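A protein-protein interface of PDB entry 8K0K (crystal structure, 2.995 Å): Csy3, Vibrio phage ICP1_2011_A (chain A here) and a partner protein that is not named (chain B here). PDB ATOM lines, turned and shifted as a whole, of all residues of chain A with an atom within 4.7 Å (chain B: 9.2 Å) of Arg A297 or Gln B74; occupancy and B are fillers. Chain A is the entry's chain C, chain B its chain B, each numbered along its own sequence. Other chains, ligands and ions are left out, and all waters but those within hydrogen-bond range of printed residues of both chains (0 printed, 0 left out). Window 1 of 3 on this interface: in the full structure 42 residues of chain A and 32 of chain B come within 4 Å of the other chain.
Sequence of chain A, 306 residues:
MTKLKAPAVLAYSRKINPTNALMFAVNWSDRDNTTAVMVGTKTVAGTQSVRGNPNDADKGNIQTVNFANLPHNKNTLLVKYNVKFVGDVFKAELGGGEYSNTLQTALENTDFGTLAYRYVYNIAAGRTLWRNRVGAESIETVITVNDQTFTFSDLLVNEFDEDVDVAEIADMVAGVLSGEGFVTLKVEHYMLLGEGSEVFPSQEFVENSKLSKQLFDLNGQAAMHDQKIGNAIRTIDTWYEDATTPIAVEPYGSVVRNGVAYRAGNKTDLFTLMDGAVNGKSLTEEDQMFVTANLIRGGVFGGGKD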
ATOM      1  N   SER A  13      20.181  10.124  32.641  1.00  0.00           N
ATOM      2  CA  SER A  13      18.839  10.461  33.082  1.00  0.00           C
ATOM      3  C   SER A  13      18.162  11.358  32.051  1.00  0.00           C
ATOM      4  O   SER A  13      18.819  12.031  31.251  1.00  0.00           O
ATOM      5  CB  SER A  13      18.868  11.150  34.447  1.00  0.00           C
ATOM      6  OG  SER A  13      19.564  12.383  34.386  1.00  0.00           O
ATOM      7  N   ARG A  14      16.832  11.354  32.067  1.00  0.00           N
ATOM      8  CA  ARG A  14      16.090  12.240  31.185  1.00  0.00           C
ATOM      9  C   ARG A  14      16.267  13.689  31.629  1.00  0.00           C
ATOM     10  O   ARG A  14      16.443  13.987  32.816  1.00  0.00           O
ATOM     11  CB  ARG A  14      14.604  11.865  31.158  1.00  0.00           C
ATOM     12  CG  ARG A  14      13.754  12.550  32.227  1.00  0.00           C
ATOM     13  CD  ARG A  14      12.268  12.254  32.062  1.00  0.00           C
ATOM     14  NE  ARG A  14      11.938  10.874  32.404  1.00  0.00           N
ATOM     15  CZ  ARG A  14      11.671  10.455  33.638  1.00  0.00           C
ATOM     16  NH1 ARG A  14      11.697  11.309  34.654  1.00  0.00           N
ATOM     17  NH2 ARG A  14      11.377   9.178  33.857  1.00  0.00           N
ATOM     18  N   ARG A 234       9.471  15.329  22.789  1.00  0.00           N
ATOM     19  CA  ARG A 234      10.710  14.968  22.106  1.00  0.00           C
ATOM     20  C   ARG A 234      10.492  14.493  20.668  1.00  0.00           C
ATOM     21  O   ARG A 234      11.447  14.034  20.031  1.00  0.00           O
ATOM     22  CB  ARG A 234      11.471  13.911  22.917  1.00  0.00           C
ATOM     23  CG  ARG A 234      11.169  12.461  22.575  1.00  0.00           C
ATOM     24  CD  ARG A 234      11.920  11.523  23.506  1.00  0.00           C
ATOM     25  NE  ARG A 234      11.004  10.834  24.408  1.00  0.00           N
ATOM     26  CZ  ARG A 234      10.561   9.597  24.211  1.00  0.00           C
ATOM     27  NH1 ARG A 234       9.720   9.046  25.077  1.00  0.00           N
ATOM     28  NH2 ARG A 234      10.965   8.905  23.151  1.00  0.00           N
ATOM     29  N   VAL A 249      12.381  11.093  19.426  1.00  0.00           N
ATOM     30  CA  VAL A 249      13.790  10.734  19.542  1.00  0.00           C
ATOM     31  C   VAL A 249      13.890   9.325  20.107  1.00  0.00           C
ATOM     32  O   VAL A 249      13.606   9.093  21.287  1.00  0.00           O
ATOM     33  CB  VAL A 249      14.560  11.729  20.427  1.00  0.00           C
ATOM     34  CG1 VAL A 249      16.002  11.283  20.572  1.00  0.00           C
ATOM     35  CG2 VAL A 249      14.489  13.126  19.844  1.00  0.00           C
ATOM     36  N   GLU A 250      14.281   8.373  19.261  1.00  0.00           N
ATOM     37  CA  GLU A 250      14.431   6.991  19.664  1.00  0.00           C
ATOM     38  C   GLU A 250      15.743   6.474  19.094  1.00  0.00           C
ATOM     39  O   GLU A 250      16.081   6.784  17.944  1.00  0.00           O
ATOM     40  CB  GLU A 250      13.266   6.115  19.175  1.00  0.00           C
ATOM     41  CG  GLU A 250      11.879   6.590  19.616  1.00  0.00           C
ATOM     42  CD  GLU A 250      11.579   6.312  21.088  1.00  0.00           C
ATOM     43  OE1 GLU A 250      12.358   5.578  21.735  1.00  0.00           O
ATOM     44  OE2 GLU A 250      10.556   6.824  21.599  1.00  0.00           O
ATOM     45  N   PRO A 251      16.500   5.698  19.871  1.00  0.00           N
ATOM     46  CA  PRO A 251      17.780   5.174  19.366  1.00  0.00           C
ATOM     47  C   PRO A 251      17.674   4.403  18.059  1.00  0.00           C
ATOM     48  O   PRO A 251      18.646   4.373  17.297  1.00  0.00           O
ATOM     49  CB  PRO A 251      18.267   4.273  20.512  1.00  0.00           C
ATOM     50  CG  PRO A 251      17.097   4.128  21.445  1.00  0.00           C
ATOM     51  CD  PRO A 251      16.293   5.369  21.289  1.00  0.00           C
ATOM     52  N   PHE A 271      23.506   3.840  17.994  1.00  0.00           N
ATOM     53  CA  PHE A 271      24.711   3.135  18.410  1.00  0.00           C
ATOM     54  C   PHE A 271      25.804   3.211  17.351  1.00  0.00           C
ATOM     55  O   PHE A 271      26.975   3.426  17.683  1.00  0.00           O
ATOM     56  CB  PHE A 271      24.355   1.692  18.755  1.00  0.00           C
ATOM     57  CG  PHE A 271      23.291   1.589  19.809  1.00  0.00           C
ATOM     58  CD1 PHE A 271      23.359   2.376  20.951  1.00  0.00           C
ATOM     59  CD2 PHE A 271      22.201   0.748  19.646  1.00  0.00           C
ATOM     60  CE1 PHE A 271      22.381   2.306  21.922  1.00  0.00           C
ATOM     61  CE2 PHE A 271      21.216   0.676  20.616  1.00  0.00           C
ATOM     62  CZ  PHE A 271      21.308   1.455  21.755  1.00  0.00           C
ATOM     63  N   ALA A 293      20.082  14.565  21.414  1.00  0.00           N
ATOM     64  CA  ALA A 293      18.683  14.460  21.806  1.00  0.00           C
ATOM     65  C   ALA A 293      18.389  13.108  22.432  1.00  0.00           C
ATOM     66  O   ALA A 293      17.537  13.013  23.319  1.00  0.00           O
ATOM     67  CB  ALA A 293      17.775  14.705  20.604  1.00  0.00           C
ATOM     68  N   ASN A 294      19.078  12.055  21.987  1.00  0.00           N
ATOM     69  CA  ASN A 294      18.974  10.773  22.678  1.00  0.00           C
ATOM     70  C   ASN A 294      19.537  10.866  24.090  1.00  0.00           C
ATOM     71  O   ASN A 294      18.996  10.261  25.023  1.00  0.00           O
ATOM     72  CB  ASN A 294      19.688   9.678  21.887  1.00  0.00           C
ATOM     73  CG  ASN A 294      18.797   9.036  20.845  1.00  0.00           C
ATOM     74  OD1 ASN A 294      18.048   8.105  21.140  1.00  0.00           O
ATOM     75  ND2 ASN A 294      18.872   9.528  19.617  1.00  0.00           N
ATOM     76  N   LEU A 295      20.630  11.612  24.265  1.00  0.00           N
ATOM     77  CA  LEU A 295      21.163  11.819  25.613  1.00  0.00           C
ATOM     78  C   LEU A 295      20.192  12.616  26.477  1.00  0.00           C
ATOM     79  O   LEU A 295      20.087  12.378  27.686  1.00  0.00           O
ATOM     80  CB  LEU A 295      22.518  12.527  25.562  1.00  0.00           C
ATOM     81  CG  LEU A 295      23.782  11.767  25.147  1.00  0.00           C
ATOM     82  CD1 LEU A 295      24.918  12.111  26.094  1.00  0.00           C
ATOM     83  CD2 LEU A 295      23.557  10.269  25.093  1.00  0.00           C
ATOM     84  N   ILE A 296      19.500  13.586  25.878  1.00  0.00           N
ATOM     85  CA  ILE A 296      18.497  14.363  26.604  1.00  0.00           C
ATOM     86  C   ILE A 296      17.311  13.481  26.973  1.00  0.00           C
ATOM     87  O   ILE A 296      16.716  13.622  28.050  1.00  0.00           O
ATOM     88  CB  ILE A 296      18.063  15.582  25.768  1.00  0.00           C
ATOM     89  CG1 ILE A 296      19.228  16.561  25.602  1.00  0.00           C
ATOM     90  CG2 ILE A 296      16.869  16.283  26.402  1.00  0.00           C
ATOM     91  CD1 ILE A 296      18.891  17.777  24.768  1.00  0.00           C
ATOM     92  N   ARG A 297      16.956  12.552  26.083  1.00  0.00           N
ATOM     93  CA  ARG A 297      15.898  11.595  26.372  1.00  0.00           C
ATOM     94  C   ARG A 297      16.216  10.789  27.619  1.00  0.00           C
ATOM     95  O   ARG A 297      15.318  10.457  28.403  1.00  0.00           O
ATOM     96  CB  ARG A 297      15.706  10.658  25.182  1.00  0.00           C
ATOM     97  CG  ARG A 297      14.504   9.761  25.313  1.00  0.00           C
ATOM     98  CD  ARG A 297      14.564   8.586  24.370  1.00  0.00           C
ATOM     99  NE  ARG A 297      14.728   7.343  25.112  1.00  0.00           N
ATOM    100  CZ  ARG A 297      14.240   6.172  24.721  1.00  0.00           C
ATOM    101  NH1 ARG A 297      13.549   6.085  23.595  1.00  0.00           N
ATOM    102  NH2 ARG A 297      14.437   5.091  25.463  1.00  0.00           N
ATOM    103  N   GLY A 298      17.489  10.482  27.829  1.00  0.00           N
ATOM    104  CA  GLY A 298      17.881   9.513  28.825  1.00  0.00           C
ATOM    105  C   GLY A 298      17.744   8.101  28.290  1.00  0.00           C
ATOM    106  O   GLY A 298      17.199   7.851  27.213  1.00  0.00           O
ATOM    107  N   GLY A 299      18.259   7.160  29.062  1.00  0.00           N
ATOM    108  CA  GLY A 299      18.181   5.766  28.682  1.00  0.00           C
ATOM    109  C   GLY A 299      19.219   4.945  29.406  1.00  0.00           C
ATOM    110  O   GLY A 299      20.176   5.462  29.984  1.00  0.00           O
ATOM    111  N   VAL A 300      19.001   3.641  29.363  1.00  0.00           N
ATOM    112  CA  VAL A 300      19.932   2.650  29.887  1.00  0.00           C
ATOM    113  C   VAL A 300      20.332   1.791  28.694  1.00  0.00           C
ATOM    114  O   VAL A 300      19.719   0.757  28.406  1.00  0.00           O
ATOM    115  CB  VAL A 300      19.315   1.816  31.013  1.00  0.00           C
ATOM    116  CG1 VAL A 300      20.273   0.725  31.478  1.00  0.00           C
ATOM    117  CG2 VAL A 300      18.921   2.723  32.171  1.00  0.00           C
ATOM    118  N   PHE A 301      21.355   2.230  27.962  1.00  0.00           N
ATOM    119  CA  PHE A 301      21.765   1.571  26.727  1.00  0.00           C
ATOM    120  C   PHE A 301      22.705   0.420  27.070  1.00  0.00           C
ATOM    121  O   PHE A 301      23.801   0.639  27.595  1.00  0.00           O
ATOM    122  CB  PHE A 301      22.419   2.584  25.791  1.00  0.00           C
ATOM    123  CG  PHE A 301      21.685   3.901  25.719  1.00  0.00           C
ATOM    124  CD1 PHE A 301      20.443   3.984  25.107  1.00  0.00           C
ATOM    125  CD2 PHE A 301      22.231   5.052  26.268  1.00  0.00           C
ATOM    126  CE1 PHE A 301      19.764   5.189  25.045  1.00  0.00           C
ATOM    127  CE2 PHE A 301      21.553   6.262  26.207  1.00  0.00           C
ATOM    128  CZ  PHE A 301      20.320   6.328  25.594  1.00  0.00           C
ATOM    129  N   GLY A 302      22.269  -0.807  26.778  1.00  0.00           N
ATOM    130  CA  GLY A 302      23.000  -1.997  27.168  1.00  0.00           C
ATOM    131  C   GLY A 302      23.548  -2.805  26.011  1.00  0.00           C
ATOM    132  O   GLY A 302      23.096  -2.660  24.871  1.00  0.00           O
ATOM    133  N   LYS B  70       5.041   1.097  29.018  1.00  0.00           N
ATOM    134  CA  LYS B  70       5.418   0.637  27.683  1.00  0.00           C
ATOM    135  C   LYS B  70       6.926   0.767  27.507  1.00  0.00           C
ATOM    136  O   LYS B  70       7.456   1.879  27.405  1.00  0.00           O
ATOM    137  CB  LYS B  70       4.670   1.425  26.611  1.00  0.00           C
ATOM    138  CG  LYS B  70       3.534   0.655  25.957  1.00  0.00           C
ATOM    139  CD  LYS B  70       3.360   1.063  24.500  1.00  0.00           C
ATOM    140  CE  LYS B  70       2.363   0.160  23.787  1.00  0.00           C
ATOM    141  NZ  LYS B  70       2.482   0.237  22.302  1.00  0.00           N
ATOM    142  N   PHE B  71       7.617  -0.367  27.453  1.00  0.00           N
ATOM    143  CA  PHE B  71       9.065  -0.356  27.303  1.00  0.00           C
ATOM    144  C   PHE B  71       9.460   0.075  25.895  1.00  0.00           C
ATOM    145  O   PHE B  71       8.915  -0.420  24.903  1.00  0.00           O
ATOM    146  CB  PHE B  71       9.641  -1.740  27.610  1.00  0.00           C
ATOM    147  CG  PHE B  71       9.933  -1.976  29.069  1.00  0.00           C
ATOM    148  CD1 PHE B  71       9.312  -1.226  30.050  1.00  0.00           C
ATOM    149  CD2 PHE B  71      10.847  -2.943  29.454  1.00  0.00           C
ATOM    150  CE1 PHE B  71       9.590  -1.444  31.386  1.00  0.00           C
ATOM    151  CE2 PHE B  71      11.130  -3.160  30.787  1.00  0.00           C
ATOM    152  CZ  PHE B  71      10.499  -2.410  31.753  1.00  0.00           C
ATOM    153  N   ALA B  72      10.416   0.997  25.813  1.00  0.00           N
ATOM    154  CA  ALA B  72      10.991   1.441  24.551  1.00  0.00           C
ATOM    155  C   ALA B  72      12.343   0.772  24.323  1.00  0.00           C
ATOM    156  O   ALA B  72      13.089   0.508  25.270  1.00  0.00           O
ATOM    157  CB  ALA B  72      11.153   2.962  24.531  1.00  0.00           C
ATOM    158  N   TRP B  73      12.650   0.506  23.050  1.00  0.00           N
ATOM    159  CA  TRP B  73      13.894  -0.168  22.692  1.00  0.00           C
ATOM    160  C   TRP B  73      15.100   0.656  23.124  1.00  0.00           C
ATOM    161  O   TRP B  73      15.088   1.888  23.061  1.00  0.00           O
ATOM    162  CB  TRP B  73      13.952  -0.422  21.193  1.00  0.00           C
ATOM    163  CG  TRP B  73      13.042  -1.504  20.737  1.00  0.00           C
ATOM    164  CD1 TRP B  73      11.864  -1.358  20.063  1.00  0.00           C
ATOM    165  CD2 TRP B  73      13.234  -2.908  20.911  1.00  0.00           C
ATOM    166  NE1 TRP B  73      11.310  -2.589  19.807  1.00  0.00           N
ATOM    167  CE2 TRP B  73      12.132  -3.558  20.319  1.00  0.00           C
ATOM    168  CE3 TRP B  73      14.231  -3.681  21.510  1.00  0.00           C
ATOM    169  CZ2 TRP B  73      12.001  -4.944  20.312  1.00  0.00           C
ATOM    170  CZ3 TRP B  73      14.099  -5.054  21.500  1.00  0.00           C
ATOM    171  CH2 TRP B  73      12.994  -5.672  20.904  1.00  0.00           C
ATOM    172  N   GLN B  74      16.154  -0.037  23.552  1.00  0.00           N
ATOM    173  CA  GLN B  74      17.189   0.634  24.326  1.00  0.00           C
ATOM    174  C   GLN B  74      18.569   0.003  24.184  1.00  0.00           C
ATOM    175  O   GLN B  74      19.573   0.639  24.517  1.00  0.00           O
ATOM    176  CB  GLN B  74      16.781   0.640  25.797  1.00  0.00           C
ATOM    177  CG  GLN B  74      16.929   1.971  26.466  1.00  0.00           C
ATOM    178  CD  GLN B  74      16.314   1.976  27.842  1.00  0.00           C
ATOM    179  OE1 GLN B  74      15.895   3.020  28.336  1.00  0.00           O
ATOM    180  NE2 GLN B  74      16.253   0.805  28.470  1.00  0.00           N
ATOM    181  N   ASP B  75      18.637  -1.234  23.706  1.00  0.00           N
ATOM    182  CA  ASP B  75      19.878  -1.991  23.708  1.00  0.00           C
ATOM    183  C   ASP B  75      20.401  -2.200  22.293  1.00  0.00           C
ATOM    184  O   ASP B  75      19.639  -2.200  21.321  1.00  0.00           O
ATOM    185  CB  ASP B  75      19.691  -3.347  24.396  1.00  0.00           C
ATOM    186  CG  ASP B  75      19.378  -3.213  25.873  1.00  0.00           C
ATOM    187  OD1 ASP B  75      19.854  -2.239  26.500  1.00  0.00           O
ATOM    188  OD2 ASP B  75      18.653  -4.081  26.404  1.00  0.00           O
ATOM    189  N   ARG B  76      21.716  -2.379  22.196  1.00  0.00           N
ATOM    190  CA  ARG B  76      22.374  -2.623  20.924  1.00  0.00           C
ATOM    191  C   ARG B  76      21.984  -3.991  20.369  1.00  0.00           C
ATOM    192  O   ARG B  76      21.522  -4.880  21.088  1.00  0.00           O
ATOM    193  CB  ARG B  76      23.891  -2.533  21.091  1.00  0.00           C
ATOM    194  CG  ARG B  76      24.360  -1.227  21.713  1.00  0.00           C
ATOM    195  CD  ARG B  76      25.827  -1.284  22.122  1.00  0.00           C
ATOM    196  NE  ARG B  76      26.361   0.049  22.394  1.00  0.00           N
ATOM    197  CZ  ARG B  76      27.107   0.747  21.540  1.00  0.00           C
ATOM    198  NH1 ARG B  76      27.422   0.234  20.357  1.00  0.00           N
ATOM    199  NH2 ARG B  76      27.542   1.955  21.869  1.00  0.00           N
ATOM    200  N   GLY B  77      22.174  -4.151  19.062  1.00  0.00           N
ATOM    201  CA  GLY B  77      21.869  -5.413  18.417  1.00  0.00           C
ATOM    202  C   GLY B  77      20.398  -5.756  18.363  1.00  0.00           C
ATOM    203  O   GLY B  77      20.044  -6.939  18.335  1.00  0.00           O
ATOM    204  N   ASN B  78      19.524  -4.750  18.344  1.00  0.00           N
ATOM    205  CA  ASN B  78      18.085  -4.973  18.293  1.00  0.00           C
ATOM    206  C   ASN B  78      17.428  -4.293  17.097  1.00  0.00           C
ATOM    207  O   ASN B  78      16.193  -4.277  17.011  1.00  0.00           O
ATOM    208  CB  ASN B  78      17.426  -4.500  19.596  1.00  0.00           C
ATOM    209  CG  ASN B  78      17.593  -5.499  20.736  1.00  0.00           C
ATOM    210  OD1 ASN B  78      17.336  -6.694  20.577  1.00  0.00           O
ATOM    211  ND2 ASN B  78      18.028  -5.010  21.894  1.00  0.00           N
ATOM    212  N   GLY B  79      18.218  -3.738  16.171  1.00  0.00           N
ATOM    213  CA  GLY B  79      17.644  -3.050  15.025  1.00  0.00           C
ATOM    214  C   GLY B  79      16.781  -3.942  14.157  1.00  0.00           C
ATOM    215  O   GLY B  79      15.775  -3.490  13.601  1.00  0.00           O
ATOM    216  N   LYS B  81      14.721  -5.806  15.192  1.00  0.00           N
ATOM    217  CA  LYS B  81      13.512  -6.061  15.962  1.00  0.00           C
ATOM    218  C   LYS B  81      12.816  -4.800  16.454  1.00  0.00           C
ATOM    219  O   LYS B  81      11.766  -4.913  17.096  1.00  0.00           O
ATOM    220  CB  LYS B  81      13.823  -6.953  17.177  1.00  0.00           C
ATOM    221  CG  LYS B  81      14.021  -8.426  16.856  1.00  0.00           C
ATOM    222  CD  LYS B  81      14.258  -9.239  18.124  1.00  0.00           C
ATOM    223  CE  LYS B  81      15.526  -8.792  18.832  1.00  0.00           C
ATOM    224  NZ  LYS B  81      15.788  -9.575  20.072  1.00  0.00           N
ATOM    225  N   ALA B  82      13.358  -3.615  16.188  1.00  0.00           N
ATOM    226  CA  ALA B  82      12.784  -2.368  16.672  1.00  0.00           C
ATOM    227  C   ALA B  82      11.512  -1.968  15.936  1.00  0.00           C
ATOM    228  O   ALA B  82      10.966  -0.892  16.213  1.00  0.00           O
ATOM    229  CB  ALA B  82      13.818  -1.249  16.563  1.00  0.00           C
ATOM    230  N   SER B  86       8.498  -3.608  22.073  1.00  0.00           N
ATOM    231  CA  SER B  86       9.610  -4.120  22.856  1.00  0.00           C
ATOM    232  C   SER B  86       9.105  -5.060  23.946  1.00  0.00           C
ATOM    233  O   SER B  86       8.061  -4.798  24.558  1.00  0.00           O
ATOM    234  CB  SER B  86      10.391  -2.969  23.489  1.00  0.00           C
ATOM    235  OG  SER B  86      11.185  -3.432  24.568  1.00  0.00           O
ATOM    236  N   PRO B  87       9.811  -6.162  24.213  1.00  0.00           N
ATOM    237  CA  PRO B  87       9.448  -7.012  25.350  1.00  0.00           C
ATOM    238  C   PRO B  87       9.480  -6.211  26.640  1.00  0.00           C
ATOM    239  O   PRO B  87      10.052  -5.120  26.719  1.00  0.00           O
ATOM    240  CB  PRO B  87      10.516  -8.110  25.335  1.00  0.00           C
ATOM    241  CG  PRO B  87      10.987  -8.146  23.923  1.00  0.00           C
ATOM    242  CD  PRO B  87      10.938  -6.720  23.452  1.00  0.00           C
ATOM    243  N   LYS B  91       6.891  -2.839  35.893  1.00  0.00           N
ATOM    244  CA  LYS B  91       7.422  -1.623  36.510  1.00  0.00           C
ATOM    245  C   LYS B  91       6.262  -0.735  36.943  1.00  0.00           C
ATOM    246  O   LYS B  91       6.004   0.313  36.347  1.00  0.00           O
ATOM    247  CB  LYS B  91       8.346  -0.889  35.539  1.00  0.00           C
ATOM    248  CG  LYS B  91       9.145   0.248  36.157  1.00  0.00           C
ATOM    249  CD  LYS B  91       9.970   0.988  35.112  1.00  0.00           C
ATOM    250  CE  LYS B  91      10.731   2.151  35.742  1.00  0.00           C
ATOM    251  NZ  LYS B  91      11.424   2.994  34.727  1.00  0.00           N
ATOM    252  N   ARG B 125      14.435  13.908  42.631  1.00  0.00           N
ATOM    253  CA  ARG B 125      13.206  13.146  42.480  1.00  0.00           C
ATOM    254  C   ARG B 125      12.842  12.543  43.833  1.00  0.00           C
ATOM    255  O   ARG B 125      13.538  12.742  44.834  1.00  0.00           O
ATOM    256  CB  ARG B 125      13.357  12.056  41.413  1.00  0.00           C
ATOM    257  CG  ARG B 125      13.163  12.540  39.988  1.00  0.00           C
ATOM    258  CD  ARG B 125      14.439  12.420  39.194  1.00  0.00           C
ATOM    259  NE  ARG B 125      14.414  11.304  38.255  1.00  0.00           N
ATOM    260  CZ  ARG B 125      14.494  11.442  36.935  1.00  0.00           C
ATOM    261  NH1 ARG B 125      14.607  12.649  36.398  1.00  0.00           N
ATOM    262  NH2 ARG B 125      14.470  10.374  36.149  1.00  0.00           N
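The backbone carbonyl oxygen (O) of Asp B75 lies within hydrogen-bond range of the side-chain amide nitrogen (ND2) of Asn B78 (3.3 Å).
NH1 of Arg A297 lies within salt-bridge range of OE2 of Glu A250 (3.7 Å).
Of the 17 printed residues of chain A, 8 touch a printed residue of chain B.
Along chain A the printed residues that touch a printed residue of chain B span positions 14 to 302.
Printed residues of chain B that touch a printed residue of chain A: Trp B73, Gln B74, Asp B75, Arg B76 and Arg B125.
Among the printed residues, no Asp or Glu carboxylate lies within 4 Å of a Lys or Arg side-chain nitrogen of the other chain.
OE1 of Gln B74 lies within hydrogen-bond range of N of Val A300.
OD1 of Asp B75 is in hydrogen-bond range of N of Gly A302 (2.8 Å).
N of Arg B76 is in hydrogen-bond range of O of Gly A302, 3.0 Å away.
NH1 of Arg A14 sits close to NH2 of Arg B125, at 3.3 Å.
Of the printed residues of chain B, Arg A14 touches Arg B125 (3.3 Å).
Arg A297 touches one residue of chain B.
No residue of chain B comes within 4 Å of Gly A298.
Of chain B, only Gln B74 and Asp B75 come within 4 Å of Val A300.
Printed residues of chain B within 4 Å of Gly A302: Gln B74, Asp B75 and Arg B76.
Printed residues of chain A within 4 Å of Gln B74: Phe A271 (3.4 Å), Arg A297 (3.8 Å), Gly A299 (3.6 Å), Val A300 (3.3 Å), Phe A301 (3.2 Å) and Gly A302 (3.8 Å).
Of the printed residues of chain A, Asp B75 touches Phe A271 (3.4 Å), Val A300 (3.6 Å), Phe A301 (3.9 Å) and Gly A302 (2.8 Å).
The nearest residue of chain B that does not touch Arg A297 is Ala B72 (4.02 Å).
The nearest printed residue of chain B that does not touch Gly A302 is Gly B77 (6.1 Å).
Among the printed residues, merely in contact across the chains: Phe A301 with Gln B74 (3.2 Å), Phe A271 with Asp B75 (3.4 Å), Phe A271 with Gln B74 (3.4 Å), Pro A251 with Trp B73 (3.4 Å), Phe A271 with Arg B76 (3.5 Å), Val A300 with Asp B75 (3.6 Å), Gly A299 with Gln B74 (3.6 Å), Gly A302 with Gln B74 (3.8 Å), Arg A297 with Gln B74 (3.8 Å) and Phe A301 with Asp B75 (3.9 Å).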
